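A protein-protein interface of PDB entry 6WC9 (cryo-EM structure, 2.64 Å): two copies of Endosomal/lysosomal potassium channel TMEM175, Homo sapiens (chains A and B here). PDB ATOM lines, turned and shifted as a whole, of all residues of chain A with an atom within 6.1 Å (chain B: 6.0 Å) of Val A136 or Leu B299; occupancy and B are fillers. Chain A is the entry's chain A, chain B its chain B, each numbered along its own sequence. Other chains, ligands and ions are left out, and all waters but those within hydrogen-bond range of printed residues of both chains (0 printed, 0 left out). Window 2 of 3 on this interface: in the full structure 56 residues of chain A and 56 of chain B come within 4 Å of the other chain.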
ATOM      1  N   LEU A 129     -18.750  -1.454   4.559  1.00  0.00           N
ATOM      2  CA  LEU A 129     -17.501  -1.604   3.824  1.00  0.00           C
ATOM      3  C   LEU A 129     -16.873  -2.970   4.073  1.00  0.00           C
ATOM      4  O   LEU A 129     -16.324  -3.587   3.155  1.00  0.00           O
ATOM      5  CB  LEU A 129     -16.543  -0.485   4.225  1.00  0.00           C
ATOM      6  CG  LEU A 129     -15.477  -0.085   3.214  1.00  0.00           C
ATOM      7  CD1 LEU A 129     -15.225   1.393   3.314  1.00  0.00           C
ATOM      8  CD2 LEU A 129     -14.200  -0.854   3.456  1.00  0.00           C
ATOM      9  N   PHE A 133     -16.442  -5.547   0.947  1.00  0.00           N
ATOM     10  CA  PHE A 133     -15.109  -5.978   0.549  1.00  0.00           C
ATOM     11  C   PHE A 133     -14.556  -6.939   1.593  1.00  0.00           C
ATOM     12  O   PHE A 133     -13.695  -6.558   2.395  1.00  0.00           O
ATOM     13  CB  PHE A 133     -14.181  -4.774   0.389  1.00  0.00           C
ATOM     14  CG  PHE A 133     -14.627  -3.809  -0.662  1.00  0.00           C
ATOM     15  CD1 PHE A 133     -14.124  -3.884  -1.945  1.00  0.00           C
ATOM     16  CD2 PHE A 133     -15.555  -2.829  -0.367  1.00  0.00           C
ATOM     17  CE1 PHE A 133     -14.537  -3.001  -2.908  1.00  0.00           C
ATOM     18  CE2 PHE A 133     -15.968  -1.946  -1.329  1.00  0.00           C
ATOM     19  CZ  PHE A 133     -15.460  -2.031  -2.601  1.00  0.00           C
ATOM     20  N   PRO A 134     -15.022  -8.191   1.621  1.00  0.00           N
ATOM     21  CA  PRO A 134     -14.612  -9.109   2.690  1.00  0.00           C
ATOM     22  C   PRO A 134     -13.234  -9.720   2.501  1.00  0.00           C
ATOM     23  O   PRO A 134     -12.781 -10.455   3.389  1.00  0.00           O
ATOM     24  CB  PRO A 134     -15.695 -10.189   2.642  1.00  0.00           C
ATOM     25  CG  PRO A 134     -16.100 -10.225   1.218  1.00  0.00           C
ATOM     26  CD  PRO A 134     -15.986  -8.821   0.702  1.00  0.00           C
ATOM     27  N   ASP A 135     -12.558  -9.450   1.387  1.00  0.00           N
ATOM     28  CA  ASP A 135     -11.248 -10.037   1.134  1.00  0.00           C
ATOM     29  C   ASP A 135     -10.105  -9.127   1.565  1.00  0.00           C
ATOM     30  O   ASP A 135      -9.095  -9.612   2.085  1.00  0.00           O
ATOM     31  CB  ASP A 135     -11.106 -10.373  -0.352  1.00  0.00           C
ATOM     32  CG  ASP A 135     -11.228 -11.863  -0.633  1.00  0.00           C
ATOM     33  OD1 ASP A 135     -10.922 -12.276  -1.771  1.00  0.00           O
ATOM     34  OD2 ASP A 135     -11.635 -12.618   0.273  1.00  0.00           O
ATOM     35  N   VAL A 136     -10.235  -7.820   1.361  1.00  0.00           N
ATOM     36  CA  VAL A 136      -9.176  -6.877   1.714  1.00  0.00           C
ATOM     37  C   VAL A 136      -9.273  -6.568   3.205  1.00  0.00           C
ATOM     38  O   VAL A 136     -10.385  -6.471   3.743  1.00  0.00           O
ATOM     39  CB  VAL A 136      -9.262  -5.598   0.869  1.00  0.00           C
ATOM     40  CG1 VAL A 136      -9.458  -5.944  -0.596  1.00  0.00           C
ATOM     41  CG2 VAL A 136     -10.381  -4.710   1.363  1.00  0.00           C
ATOM     42  N   PRO A 137      -8.148  -6.398   3.909  1.00  0.00           N
ATOM     43  CA  PRO A 137      -8.217  -6.222   5.366  1.00  0.00           C
ATOM     44  C   PRO A 137      -8.513  -4.804   5.817  1.00  0.00           C
ATOM     45  O   PRO A 137      -8.688  -4.586   7.022  1.00  0.00           O
ATOM     46  CB  PRO A 137      -6.826  -6.663   5.832  1.00  0.00           C
ATOM     47  CG  PRO A 137      -5.934  -6.335   4.680  1.00  0.00           C
ATOM     48  CD  PRO A 137      -6.757  -6.434   3.425  1.00  0.00           C
ATOM     49  N   LEU A 138      -8.570  -3.834   4.904  1.00  0.00           N
ATOM     50  CA  LEU A 138      -8.797  -2.453   5.315  1.00  0.00           C
ATOM     51  C   LEU A 138     -10.175  -2.263   5.932  1.00  0.00           C
ATOM     52  O   LEU A 138     -10.344  -1.430   6.832  1.00  0.00           O
ATOM     53  CB  LEU A 138      -8.620  -1.521   4.119  1.00  0.00           C
ATOM     54  CG  LEU A 138      -8.649  -0.030   4.436  1.00  0.00           C
ATOM     55  CD1 LEU A 138      -7.380   0.628   3.951  1.00  0.00           C
ATOM     56  CD2 LEU A 138      -9.864   0.630   3.811  1.00  0.00           C
ATOM     57  N   GLY A 139     -11.171  -3.025   5.478  1.00  0.00           N
ATOM     58  CA  GLY A 139     -12.521  -2.828   5.981  1.00  0.00           C
ATOM     59  C   GLY A 139     -12.669  -3.253   7.429  1.00  0.00           C
ATOM     60  O   GLY A 139     -13.179  -2.499   8.265  1.00  0.00           O
ATOM     61  N   ILE A 140     -12.235  -4.473   7.744  1.00  0.00           N
ATOM     62  CA  ILE A 140     -12.275  -4.933   9.128  1.00  0.00           C
ATOM     63  C   ILE A 140     -11.367  -4.072   9.992  1.00  0.00           C
ATOM     64  O   ILE A 140     -11.663  -3.813  11.163  1.00  0.00           O
ATOM     65  CB  ILE A 140     -11.901  -6.425   9.206  1.00  0.00           C
ATOM     66  CG1 ILE A 140     -12.300  -7.005  10.564  1.00  0.00           C
ATOM     67  CG2 ILE A 140     -10.419  -6.628   8.967  1.00  0.00           C
ATOM     68  CD1 ILE A 140     -12.751  -8.449  10.498  1.00  0.00           C
ATOM     69  N   PRO B 286     -18.006   2.592  -1.731  1.00  0.00           N
ATOM     70  CA  PRO B 286     -17.451   2.139  -3.011  1.00  0.00           C
ATOM     71  C   PRO B 286     -18.030   0.802  -3.448  1.00  0.00           C
ATOM     72  O   PRO B 286     -18.238  -0.104  -2.638  1.00  0.00           O
ATOM     73  CB  PRO B 286     -15.948   2.031  -2.730  1.00  0.00           C
ATOM     74  CG  PRO B 286     -15.708   2.874  -1.552  1.00  0.00           C
ATOM     75  CD  PRO B 286     -16.951   2.850  -0.738  1.00  0.00           C
ATOM     76  N   VAL B 291     -14.103   0.275  -7.952  1.00  0.00           N
ATOM     77  CA  VAL B 291     -12.868   0.206  -7.179  1.00  0.00           C
ATOM     78  C   VAL B 291     -11.754  -0.422  -8.006  1.00  0.00           C
ATOM     79  O   VAL B 291     -10.696   0.185  -8.207  1.00  0.00           O
ATOM     80  CB  VAL B 291     -13.100  -0.558  -5.865  1.00  0.00           C
ATOM     81  CG1 VAL B 291     -11.799  -0.741  -5.109  1.00  0.00           C
ATOM     82  CG2 VAL B 291     -14.096   0.195  -5.008  1.00  0.00           C
ATOM     83  N   GLY B 297      -7.538  -1.265  -8.884  1.00  0.00           N
ATOM     84  CA  GLY B 297      -7.509  -2.237  -7.807  1.00  0.00           C
ATOM     85  C   GLY B 297      -6.954  -1.685  -6.511  1.00  0.00           C
ATOM     86  O   GLY B 297      -5.848  -2.045  -6.097  1.00  0.00           O
ATOM     87  N   SER B 298      -7.716  -0.811  -5.861  1.00  0.00           N
ATOM     88  CA  SER B 298      -7.292  -0.182  -4.616  1.00  0.00           C
ATOM     89  C   SER B 298      -8.511   0.418  -3.938  1.00  0.00           C
ATOM     90  O   SER B 298      -9.171   1.294  -4.505  1.00  0.00           O
ATOM     91  CB  SER B 298      -6.235   0.895  -4.869  1.00  0.00           C
ATOM     92  OG  SER B 298      -6.266   1.882  -3.854  1.00  0.00           O
ATOM     93  N   LEU B 299      -8.810  -0.058  -2.730  1.00  0.00           N
ATOM     94  CA  LEU B 299      -9.937   0.472  -1.975  1.00  0.00           C
ATOM     95  C   LEU B 299      -9.566   1.764  -1.260  1.00  0.00           C
ATOM     96  O   LEU B 299     -10.404   2.662  -1.113  1.00  0.00           O
ATOM     97  CB  LEU B 299     -10.419  -0.576  -0.976  1.00  0.00           C
ATOM     98  CG  LEU B 299     -11.477  -0.147   0.036  1.00  0.00           C
ATOM     99  CD1 LEU B 299     -12.781   0.162  -0.662  1.00  0.00           C
ATOM    100  CD2 LEU B 299     -11.662  -1.228   1.082  1.00  0.00           C
ATOM    101  N   VAL B 300      -8.316   1.871  -0.805  1.00  0.00           N
ATOM    102  CA  VAL B 300      -7.874   3.080  -0.118  1.00  0.00           C
ATOM    103  C   VAL B 300      -7.960   4.286  -1.042  1.00  0.00           C
ATOM    104  O   VAL B 300      -8.300   5.391  -0.604  1.00  0.00           O
ATOM    105  CB  VAL B 300      -6.447   2.880   0.432  1.00  0.00           C
ATOM    106  CG1 VAL B 300      -5.495   2.432  -0.667  1.00  0.00           C
ATOM    107  CG2 VAL B 300      -5.947   4.147   1.082  1.00  0.00           C
ATOM    108  N   ALA B 301      -7.679   4.098  -2.333  1.00  0.00           N
ATOM    109  CA  ALA B 301      -7.778   5.204  -3.278  1.00  0.00           C
ATOM    110  C   ALA B 301      -9.218   5.677  -3.416  1.00  0.00           C
ATOM    111  O   ALA B 301      -9.503   6.882  -3.355  1.00  0.00           O
ATOM    112  CB  ALA B 301      -7.222   4.777  -4.635  1.00  0.00           C
ATOM    113  N   ALA B 302     -10.145   4.738  -3.607  1.00  0.00           N
ATOM    114  CA  ALA B 302     -11.548   5.102  -3.752  1.00  0.00           C
ATOM    115  C   ALA B 302     -12.085   5.738  -2.477  1.00  0.00           C
ATOM    116  O   ALA B 302     -12.983   6.586  -2.530  1.00  0.00           O
ATOM    117  CB  ALA B 302     -12.368   3.872  -4.124  1.00  0.00           C
ATOM    118  N   LEU B 303     -11.552   5.342  -1.321  1.00  0.00           N
ATOM    119  CA  LEU B 303     -11.994   5.947  -0.071  1.00  0.00           C
ATOM    120  C   LEU B 303     -11.434   7.353   0.086  1.00  0.00           C
ATOM    121  O   LEU B 303     -12.127   8.252   0.577  1.00  0.00           O
ATOM    122  CB  LEU B 303     -11.584   5.073   1.111  1.00  0.00           C
ATOM    123  CG  LEU B 303     -12.398   3.794   1.275  1.00  0.00           C
ATOM    124  CD1 LEU B 303     -11.664   2.818   2.164  1.00  0.00           C
ATOM    125  CD2 LEU B 303     -13.768   4.104   1.838  1.00  0.00           C
ATOM    126  N   SER B 304     -10.181   7.563  -0.320  1.00  0.00           N
ATOM    127  CA  SER B 304      -9.610   8.901  -0.277  1.00  0.00           C
ATOM    128  C   SER B 304     -10.329   9.837  -1.236  1.00  0.00           C
ATOM    129  O   SER B 304     -10.439  11.038  -0.964  1.00  0.00           O
ATOM    130  CB  SER B 304      -8.120   8.843  -0.607  1.00  0.00           C
ATOM    131  OG  SER B 304      -7.899   9.029  -1.994  1.00  0.00           O
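Hydrophobic or aromatic side chains of chain B that line the printed part of chain A: Val B291, Leu B299 and Leu B303. Of the 9 printed residues of chain A, 4 touch a printed residue of chain B. Hydrophobic or aromatic side chains of chain A that line the printed part of chain B: Leu A129, Phe A133, Val A136 and Leu A138.
No position is printed for both chains.
Val A136 touches just one residue of chain B: Leu B299 (3.7 Å). Of the printed residues of chain A, Pro B286 touches Phe A133 (3.2 Å). Printed residues of chain A within 4 Å of Val B291: Phe A133. The nearest printed residue of chain B that does not touch Val A136 is Val B300 (7.2 Å). The nearest printed residue of chain A that does not touch Pro B286 is Leu A129 (4.6 Å).
Among the printed residues, pairs that only touch across the chains: Leu A129 with Leu B299 (3.5 Å), Leu A129 with Leu B303 (3.4 Å), Phe A133 with Pro B286 (3.2 Å), Phe A133 with Val B291 (3.6 Å), Phe A133 with Leu B299 (3.9 Å), Val A136 with Leu B299 (3.7 Å), Leu A138 with Leu B299 (3.8 Å) and Leu A138 with Leu B303 (3.3 Å).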
